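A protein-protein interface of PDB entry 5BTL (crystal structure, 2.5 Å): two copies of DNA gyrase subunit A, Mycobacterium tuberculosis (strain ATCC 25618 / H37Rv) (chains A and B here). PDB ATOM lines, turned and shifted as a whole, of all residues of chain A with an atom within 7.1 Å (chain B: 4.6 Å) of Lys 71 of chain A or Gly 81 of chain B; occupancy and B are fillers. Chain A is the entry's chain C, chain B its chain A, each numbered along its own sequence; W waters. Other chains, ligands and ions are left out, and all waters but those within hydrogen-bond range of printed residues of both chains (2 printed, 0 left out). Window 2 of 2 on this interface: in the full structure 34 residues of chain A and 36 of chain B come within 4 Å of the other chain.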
ATOM      1  N   PHE A  63      -6.106 -32.823   5.128  1.00  0.00           N
ATOM      2  CA  PHE A  63      -7.271 -32.178   4.529  1.00  0.00           C
ATOM      3  C   PHE A  63      -7.870 -33.083   3.457  1.00  0.00           C
ATOM      4  O   PHE A  63      -7.772 -32.801   2.261  1.00  0.00           O
ATOM      5  CB  PHE A  63      -6.892 -30.820   3.933  1.00  0.00           C
ATOM      6  CG  PHE A  63      -6.280 -29.866   4.924  1.00  0.00           C
ATOM      7  CD1 PHE A  63      -6.427 -30.062   6.289  1.00  0.00           C
ATOM      8  CD2 PHE A  63      -5.564 -28.764   4.484  1.00  0.00           C
ATOM      9  CE1 PHE A  63      -5.862 -29.183   7.195  1.00  0.00           C
ATOM     10  CE2 PHE A  63      -5.000 -27.882   5.385  1.00  0.00           C
ATOM     11  CZ  PHE A  63      -5.151 -28.090   6.742  1.00  0.00           C
ATOM     12  N   SER A  68     -13.879 -32.813   7.563  1.00  0.00           N
ATOM     13  CA  SER A  68     -14.550 -31.593   7.131  1.00  0.00           C
ATOM     14  C   SER A  68     -13.578 -30.660   6.425  1.00  0.00           C
ATOM     15  O   SER A  68     -12.370 -30.728   6.648  1.00  0.00           O
ATOM     16  CB  SER A  68     -15.195 -30.886   8.324  1.00  0.00           C
ATOM     17  OG  SER A  68     -14.232 -30.570   9.312  1.00  0.00           O
ATOM     18  N   HIS A  69     -14.113 -29.797   5.569  1.00  0.00           N
ATOM     19  CA  HIS A  69     -13.292 -28.840   4.840  1.00  0.00           C
ATOM     20  C   HIS A  69     -12.488 -27.974   5.798  1.00  0.00           C
ATOM     21  O   HIS A  69     -13.038 -27.389   6.731  1.00  0.00           O
ATOM     22  CB  HIS A  69     -14.154 -27.945   3.943  1.00  0.00           C
ATOM     23  CG  HIS A  69     -14.853 -28.677   2.840  1.00  0.00           C
ATOM     24  ND1 HIS A  69     -15.935 -29.499   3.058  1.00  0.00           N
ATOM     25  CD2 HIS A  69     -14.626 -28.696   1.505  1.00  0.00           C
ATOM     26  CE1 HIS A  69     -16.343 -30.001   1.904  1.00  0.00           C
ATOM     27  NE2 HIS A  69     -15.566 -29.529   0.948  1.00  0.00           N
ATOM     28  N   ALA A  70     -11.181 -27.911   5.572  1.00  0.00           N
ATOM     29  CA  ALA A  70     -10.319 -27.006   6.314  1.00  0.00           C
ATOM     30  C   ALA A  70     -10.372 -25.641   5.649  1.00  0.00           C
ATOM     31  O   ALA A  70     -10.653 -25.548   4.456  1.00  0.00           O
ATOM     32  CB  ALA A  70      -8.894 -27.534   6.357  1.00  0.00           C
ATOM     33  N   LYS A  71     -10.131 -24.583   6.415  1.00  0.00           N
ATOM     34  CA  LYS A  71     -10.041 -23.249   5.835  1.00  0.00           C
ATOM     35  C   LYS A  71      -8.937 -23.229   4.787  1.00  0.00           C
ATOM     36  O   LYS A  71      -7.813 -23.657   5.047  1.00  0.00           O
ATOM     37  CB  LYS A  71      -9.780 -22.200   6.915  1.00  0.00           C
ATOM     38  CG  LYS A  71     -11.011 -21.841   7.727  1.00  0.00           C
ATOM     39  CD  LYS A  71     -11.999 -21.021   6.908  1.00  0.00           C
ATOM     40  CE  LYS A  71     -13.292 -20.777   7.669  1.00  0.00           C
ATOM     41  NZ  LYS A  71     -14.305 -20.076   6.829  1.00  0.00           N
ATOM     42  N   SER A  72      -9.269 -22.734   3.598  1.00  0.00           N
ATOM     43  CA  SER A  72      -8.362 -22.801   2.460  1.00  0.00           C
ATOM     44  C   SER A  72      -7.057 -22.055   2.731  1.00  0.00           C
ATOM     45  O   SER A  72      -6.027 -22.360   2.126  1.00  0.00           O
ATOM     46  CB  SER A  72      -9.043 -22.246   1.208  1.00  0.00           C
ATOM     47  OG  SER A  72      -9.414 -20.893   1.383  1.00  0.00           O
ATOM     48  N   ALA A  73      -7.104 -21.085   3.640  1.00  0.00           N
ATOM     49  CA  ALA A  73      -5.912 -20.335   4.030  1.00  0.00           C
ATOM     50  C   ALA A  73      -4.857 -21.261   4.612  1.00  0.00           C
ATOM     51  O   ALA A  73      -3.660 -21.041   4.436  1.00  0.00           O
ATOM     52  CB  ALA A  73      -6.268 -19.251   5.033  1.00  0.00           C
ATOM     53  N   ARG A  74      -5.307 -22.300   5.310  1.00  0.00           N
ATOM     54  CA  ARG A  74      -4.392 -23.255   5.922  1.00  0.00           C
ATOM     55  C   ARG A  74      -3.665 -24.077   4.864  1.00  0.00           C
ATOM     56  O   ARG A  74      -2.508 -24.456   5.054  1.00  0.00           O
ATOM     57  CB  ARG A  74      -5.139 -24.180   6.880  1.00  0.00           C
ATOM     58  CG  ARG A  74      -5.738 -23.471   8.080  1.00  0.00           C
ATOM     59  CD  ARG A  74      -6.484 -24.448   8.962  1.00  0.00           C
ATOM     60  NE  ARG A  74      -5.593 -25.479   9.486  1.00  0.00           N
ATOM     61  CZ  ARG A  74      -5.987 -26.497  10.244  1.00  0.00           C
ATOM     62  NH1 ARG A  74      -7.266 -26.630  10.573  1.00  0.00           N
ATOM     63  NH2 ARG A  74      -5.101 -27.385  10.672  1.00  0.00           N
ATOM     64  N   SER A  75      -4.346 -24.354   3.755  1.00  0.00           N
ATOM     65  CA  SER A  75      -3.734 -25.083   2.649  1.00  0.00           C
ATOM     66  C   SER A  75      -2.704 -24.208   1.946  1.00  0.00           C
ATOM     67  O   SER A  75      -1.589 -24.653   1.670  1.00  0.00           O
ATOM     68  CB  SER A  75      -4.797 -25.555   1.657  1.00  0.00           C
ATOM     69  OG  SER A  75      -5.624 -26.547   2.237  1.00  0.00           O
ATOM     70  N   VAL A  76      -3.079 -22.963   1.667  1.00  0.00           N
ATOM     71  CA  VAL A  76      -2.162 -22.005   1.059  1.00  0.00           C
ATOM     72  C   VAL A  76      -0.930 -21.804   1.936  1.00  0.00           C
ATOM     73  O   VAL A  76       0.197 -21.831   1.447  1.00  0.00           O
ATOM     74  CB  VAL A  76      -2.844 -20.641   0.819  1.00  0.00           C
ATOM     75  CG1 VAL A  76      -1.848 -19.621   0.277  1.00  0.00           C
ATOM     76  CG2 VAL A  76      -4.007 -20.790  -0.139  1.00  0.00           C
ATOM     77  N   GLN A 112     -15.504 -25.430  -0.797  1.00  0.00           N
ATOM     78  CA  GLN A 112     -16.723 -25.066  -0.086  1.00  0.00           C
ATOM     79  C   GLN A 112     -16.831 -23.551   0.035  1.00  0.00           C
ATOM     80  O   GLN A 112     -16.032 -22.915   0.721  1.00  0.00           O
ATOM     81  CB  GLN A 112     -16.751 -25.715   1.297  1.00  0.00           C
ATOM     82  CG  GLN A 112     -17.912 -25.267   2.159  1.00  0.00           C
ATOM     83  CD  GLN A 112     -18.165 -26.197   3.329  1.00  0.00           C
ATOM     84  OE1 GLN A 112     -17.980 -25.819   4.487  1.00  0.00           O
ATOM     85  NE2 GLN A 112     -18.603 -27.418   3.034  1.00  0.00           N
ATOM     86  N   MET A 126      -9.636 -15.683   0.104  1.00  0.00           N
ATOM     87  CA  MET A 126      -9.130 -16.823   0.859  1.00  0.00           C
ATOM     88  C   MET A 126      -9.837 -17.023   2.200  1.00  0.00           C
ATOM     89  O   MET A 126     -10.097 -18.152   2.617  1.00  0.00           O
ATOM     90  CB  MET A 126      -7.630 -16.634   1.093  1.00  0.00           C
ATOM     91  CG  MET A 126      -6.912 -17.829   1.679  1.00  0.00           C
ATOM     92  SD  MET A 126      -5.133 -17.550   1.814  1.00  0.00           S
ATOM     93  CE  MET A 126      -5.076 -16.122   2.894  1.00  0.00           C
ATOM     94  N   ARG A 127     -10.156 -15.919   2.865  1.00  0.00           N
ATOM     95  CA  ARG A 127     -10.745 -15.964   4.196  1.00  0.00           C
ATOM     96  C   ARG A 127     -12.128 -16.613   4.193  1.00  0.00           C
ATOM     97  O   ARG A 127     -12.532 -17.234   5.176  1.00  0.00           O
ATOM     98  CB  ARG A 127     -10.837 -14.549   4.771  1.00  0.00           C
ATOM     99  CG  ARG A 127     -11.757 -13.630   3.980  1.00  0.00           C
ATOM    100  CD  ARG A 127     -11.654 -12.186   4.443  1.00  0.00           C
ATOM    101  NE  ARG A 127     -10.340 -11.610   4.164  1.00  0.00           N
ATOM    102  CZ  ARG A 127     -10.003 -10.351   4.428  1.00  0.00           C
ATOM    103  NH1 ARG A 127     -10.882  -9.522   4.977  1.00  0.00           N
ATOM    104  NH2 ARG A 127      -8.784  -9.920   4.139  1.00  0.00           N
ATOM    105  N   PTR A 128     -12.801 -16.566   3.050  1.00  0.00           N
ATOM    106  CA  PTR A 128     -14.221 -16.958   3.024  1.00  0.00           C
ATOM    107  C   PTR A 128     -14.411 -18.340   2.581  1.00  0.00           C
ATOM    108  O   PTR A 128     -15.551 -18.880   2.649  1.00  0.00           O
ATOM    109  CB  PTR A 128     -14.889 -16.098   1.990  1.00  0.00           C
ATOM    110  CG  PTR A 128     -14.998 -14.641   2.344  1.00  0.00           C
ATOM    111  CD1 PTR A 128     -14.450 -13.726   1.470  1.00  0.00           C
ATOM    112  CD2 PTR A 128     -15.672 -14.195   3.460  1.00  0.00           C
ATOM    113  CE1 PTR A 128     -14.548 -12.372   1.723  1.00  0.00           C
ATOM    114  CE2 PTR A 128     -15.768 -12.825   3.716  1.00  0.00           C
ATOM    115  CZ  PTR A 128     -15.212 -11.930   2.846  1.00  0.00           C
ATOM    116  OH  PTR A 128     -15.300 -10.602   3.133  1.00  0.00           O
ATOM    117  P   PTR A 128     -15.522  -9.597   1.944  1.00  0.00           P
ATOM    118  O1P PTR A 128     -16.020  -8.299   2.455  1.00  0.00           O
ATOM    119  O2P PTR A 128     -14.200  -9.401   1.174  1.00  0.00           O
ATOM    120  O3P PTR A 128     -16.596 -10.172   0.998  1.00  0.00           O
ATOM    121  N   THR A 129     -13.373 -18.993   2.109  1.00  0.00           N
ATOM    122  CA  THR A 129     -13.528 -20.323   1.526  1.00  0.00           C
ATOM    123  C   THR A 129     -12.857 -21.421   2.343  1.00  0.00           C
ATOM    124  O   THR A 129     -11.875 -21.183   3.046  1.00  0.00           O
ATOM    125  CB  THR A 129     -12.959 -20.369   0.094  1.00  0.00           C
ATOM    126  OG1 THR A 129     -11.529 -20.277   0.138  1.00  0.00           O
ATOM    127  CG2 THR A 129     -13.521 -19.227  -0.745  1.00  0.00           C
ATOM    128  N   GLU A 130     -13.406 -22.626   2.232  1.00  0.00           N
ATOM    129  CA  GLU A 130     -12.799 -23.819   2.807  1.00  0.00           C
ATOM    130  C   GLU A 130     -12.502 -24.787   1.667  1.00  0.00           C
ATOM    131  O   GLU A 130     -13.070 -24.666   0.582  1.00  0.00           O
ATOM    132  CB  GLU A 130     -13.718 -24.463   3.849  1.00  0.00           C
ATOM    133  CG  GLU A 130     -14.053 -23.559   5.022  1.00  0.00           C
ATOM    134  CD  GLU A 130     -14.938 -24.237   6.053  1.00  0.00           C
ATOM    135  OE1 GLU A 130     -15.510 -25.303   5.743  1.00  0.00           O
ATOM    136  OE2 GLU A 130     -15.063 -23.702   7.176  1.00  0.00           O
ATOM    137  N   ALA A 131     -11.616 -25.746   1.908  1.00  0.00           N
ATOM    138  CA  ALA A 131     -11.193 -26.645   0.847  1.00  0.00           C
ATOM    139  C   ALA A 131     -10.607 -27.942   1.386  1.00  0.00           C
ATOM    140  O   ALA A 131     -10.003 -27.973   2.459  1.00  0.00           O
ATOM    141  CB  ALA A 131     -10.177 -25.948  -0.047  1.00  0.00           C
ATOM    142  N   ALA B  77      -2.785 -18.282   9.339  1.00  0.00           N
ATOM    143  CA  ALA B  77      -3.721 -19.305   8.881  1.00  0.00           C
ATOM    144  C   ALA B  77      -4.223 -20.160  10.042  1.00  0.00           C
ATOM    145  O   ALA B  77      -5.402 -20.508  10.096  1.00  0.00           O
ATOM    146  CB  ALA B  77      -3.071 -20.180   7.823  1.00  0.00           C
ATOM    147  N   GLU B  78      -3.329 -20.504  10.963  1.00  0.00           N
ATOM    148  CA  GLU B  78      -3.707 -21.302  12.124  1.00  0.00           C
ATOM    149  C   GLU B  78      -4.633 -20.519  13.048  1.00  0.00           C
ATOM    150  O   GLU B  78      -5.602 -21.067  13.577  1.00  0.00           O
ATOM    151  CB  GLU B  78      -2.467 -21.760  12.894  1.00  0.00           C
ATOM    152  CG  GLU B  78      -1.974 -23.139  12.494  1.00  0.00           C
ATOM    153  CD  GLU B  78      -2.908 -24.246  12.945  1.00  0.00           C
ATOM    154  OE1 GLU B  78      -3.352 -24.218  14.115  1.00  0.00           O
ATOM    155  OE2 GLU B  78      -3.205 -25.142  12.126  1.00  0.00           O
ATOM    156  N   THR B  79      -4.331 -19.238  13.240  1.00  0.00           N
ATOM    157  CA  THR B  79      -5.166 -18.377  14.068  1.00  0.00           C
ATOM    158  C   THR B  79      -6.532 -18.199  13.418  1.00  0.00           C
ATOM    159  O   THR B  79      -7.569 -18.285  14.077  1.00  0.00           O
ATOM    160  CB  THR B  79      -4.522 -16.991  14.279  1.00  0.00           C
ATOM    161  OG1 THR B  79      -3.176 -17.144  14.745  1.00  0.00           O
ATOM    162  CG2 THR B  79      -5.320 -16.175  15.290  1.00  0.00           C
ATOM    163  N   MET B  80      -6.516 -17.969  12.110  1.00  0.00           N
ATOM    164  CA  MET B  80      -7.729 -17.743  11.337  1.00  0.00           C
ATOM    165  C   MET B  80      -8.618 -18.979  11.300  1.00  0.00           C
ATOM    166  O   MET B  80      -9.834 -18.888  11.466  1.00  0.00           O
ATOM    167  CB  MET B  80      -7.365 -17.332   9.913  1.00  0.00           C
ATOM    168  CG  MET B  80      -8.440 -16.553   9.183  1.00  0.00           C
ATOM    169  SD  MET B  80      -8.105 -16.330   7.419  1.00  0.00           S
ATOM    170  CE  MET B  80      -6.334 -16.622   7.327  1.00  0.00           C
ATOM    171  N   GLY B  81      -8.000 -20.132  11.072  1.00  0.00           N
ATOM    172  CA  GLY B  81      -8.733 -21.362  10.827  1.00  0.00           C
ATOM    173  C   GLY B  81      -9.340 -22.018  12.053  1.00  0.00           C
ATOM    174  O   GLY B  81     -10.271 -22.814  11.926  1.00  0.00           O
ATOM    175  N   ASN B  82      -8.820 -21.693  13.234  1.00  0.00           N
ATOM    176  CA  ASN B  82      -9.206 -22.389  14.459  1.00  0.00           C
ATOM    177  C   ASN B  82      -9.849 -21.509  15.528  1.00  0.00           C
ATOM    178  O   ASN B  82     -10.697 -21.981  16.286  1.00  0.00           O
ATOM    179  CB  ASN B  82      -7.984 -23.087  15.063  1.00  0.00           C
ATOM    180  CG  ASN B  82      -7.564 -24.312  14.274  1.00  0.00           C
ATOM    181  OD1 ASN B  82      -6.699 -24.238  13.400  1.00  0.00           O
ATOM    182  ND2 ASN B  82      -8.186 -25.450  14.571  1.00  0.00           N
ATOM    183  N   TYR B  83      -9.451 -20.240  15.596  1.00  0.00           N
ATOM    184  CA  TYR B  83      -9.814 -19.395  16.734  1.00  0.00           C
ATOM    185  C   TYR B  83     -10.420 -18.047  16.351  1.00  0.00           C
ATOM    186  O   TYR B  83     -11.393 -17.607  16.965  1.00  0.00           O
ATOM    187  CB  TYR B  83      -8.581 -19.163  17.611  1.00  0.00           C
ATOM    188  CG  TYR B  83      -7.822 -20.432  17.921  1.00  0.00           C
ATOM    189  CD1 TYR B  83      -8.323 -21.359  18.828  1.00  0.00           C
ATOM    190  CD2 TYR B  83      -6.606 -20.705  17.310  1.00  0.00           C
ATOM    191  CE1 TYR B  83      -7.636 -22.521  19.113  1.00  0.00           C
ATOM    192  CE2 TYR B  83      -5.912 -21.863  17.590  1.00  0.00           C
ATOM    193  CZ  TYR B  83      -6.430 -22.767  18.492  1.00  0.00           C
ATOM    194  OH  TYR B  83      -5.740 -23.922  18.773  1.00  0.00           O
ATOM    195  N   TYR B 155     -15.106 -20.902  17.766  1.00  0.00           N
ATOM    196  CA  TYR B 155     -16.238 -20.280  17.089  1.00  0.00           C
ATOM    197  C   TYR B 155     -17.136 -21.289  16.367  1.00  0.00           C
ATOM    198  O   TYR B 155     -18.230 -20.934  15.926  1.00  0.00           O
ATOM    199  CB  TYR B 155     -15.739 -19.221  16.100  1.00  0.00           C
ATOM    200  CG  TYR B 155     -14.930 -19.772  14.950  1.00  0.00           C
ATOM    201  CD1 TYR B 155     -15.543 -20.171  13.769  1.00  0.00           C
ATOM    202  CD2 TYR B 155     -13.550 -19.883  15.041  1.00  0.00           C
ATOM    203  CE1 TYR B 155     -14.804 -20.673  12.714  1.00  0.00           C
ATOM    204  CE2 TYR B 155     -12.802 -20.383  13.993  1.00  0.00           C
ATOM    205  CZ  TYR B 155     -13.433 -20.776  12.831  1.00  0.00           C
ATOM    206  OH  TYR B 155     -12.690 -21.273  11.787  1.00  0.00           O
ATOM    207  N   ARG B 158     -15.271 -26.940  17.146  1.00  0.00           N
ATOM    208  CA  ARG B 158     -14.313 -27.956  16.716  1.00  0.00           C
ATOM    209  C   ARG B 158     -13.192 -28.185  17.726  1.00  0.00           C
ATOM    210  O   ARG B 158     -12.787 -29.324  17.962  1.00  0.00           O
ATOM    211  CB  ARG B 158     -13.705 -27.556  15.369  1.00  0.00           C
ATOM    212  CG  ARG B 158     -14.593 -27.827  14.164  1.00  0.00           C
ATOM    213  CD  ARG B 158     -13.910 -27.414  12.863  1.00  0.00           C
ATOM    214  NE  ARG B 158     -12.571 -27.985  12.710  1.00  0.00           N
ATOM    215  CZ  ARG B 158     -11.434 -27.334  12.968  1.00  0.00           C
ATOM    216  NH1 ARG B 158     -11.447 -26.077  13.406  1.00  0.00           N
ATOM    217  NH2 ARG B 158     -10.270 -27.947  12.793  1.00  0.00           N
HETATM  218  O   HOH W   1      -2.779 -26.083   9.637  1.00  0.00           O
HETATM  219  O   HOH W   2      -8.800 -29.107  10.374  1.00  0.00           O
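Among the printed residues, merely in contact across the chains: Lys 71 of chain A with Gly 81 of chain B, Ala 73 of chain A with Ala 77 of chain B, Ala 73 of chain A with Met 80 of chain B, Arg 74 of chain A with Ala 77 of chain B, Arg 74 of chain A with Asn 82 of chain B and Arg 74 of chain A with Arg 158 of chain B.
Printed residues of chain B that touch a printed residue of chain A: Ala 77, Glu 78, Met 80, Gly 81, Asn 82 and Arg 158.
Among the printed residues, 7 pairs touch across the chains.
Among the printed residues, Asp or Glu carboxylates within 4 Å of a Lys or Arg side-chain nitrogen of the other chain: Arg 74 of chain A with Glu 78 of chain B.
Of chain B, only Gly 81 (3.9 Å) comes within 4 Å of Lys 71 of chain A.
Of the printed residues of chain B, Ala 73 of chain A touches Ala 77 and Met 80.
Ala 131 of chain A touches none of the printed residues of chain B.
Of the printed residues of chain A, Ala 77 of chain B touches Ala 73 (3.5 Å) and Arg 74 (3.6 Å).
Of the printed residues of chain A, Met 80 of chain B touches Ala 73.
Of the printed residues of chain A, Gly 81 of chain B touches Lys 71 (3.9 Å).
Of the printed residues of chain A, Asn 82 of chain B touches Arg 74 (3.7 Å).
Tyr 83 of chain B touches none of the printed residues of chain A.
Water W1 bridges OE2 of Glu 78 of chain B (2.7 Å) and NH2 of Arg 74 of chain A (2.9 Å).
Water W2 bridges the guanidinium group of Arg 74 of chain A (2.9 Å) and the guanidinium group of Arg 158 of chain B (3.1 Å).
The backbone carbonyl oxygen (O) of Glu 78 of chain B lies close to the side-chain amide oxygen (OD1) of Asn 82 of chain B.
The side-chain hydroxyl (OH) of Tyr 155 of chain B lies within hydrogen-bond range of the backbone carbonyl oxygen (O) of Gly 81 of chain B.
The side-chain carboxylate of Glu 130 of chain A is in salt-bridge range of the side-chain amino group of Lys 71 of chain A (3.7 Å).
The side-chain carboxylate (OE2) of Glu 78 of chain B lies within salt-bridge range of the guanidinium group (NH2) of Arg 74 of chain A, 3.3 Å away.
No position is printed for both chains.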
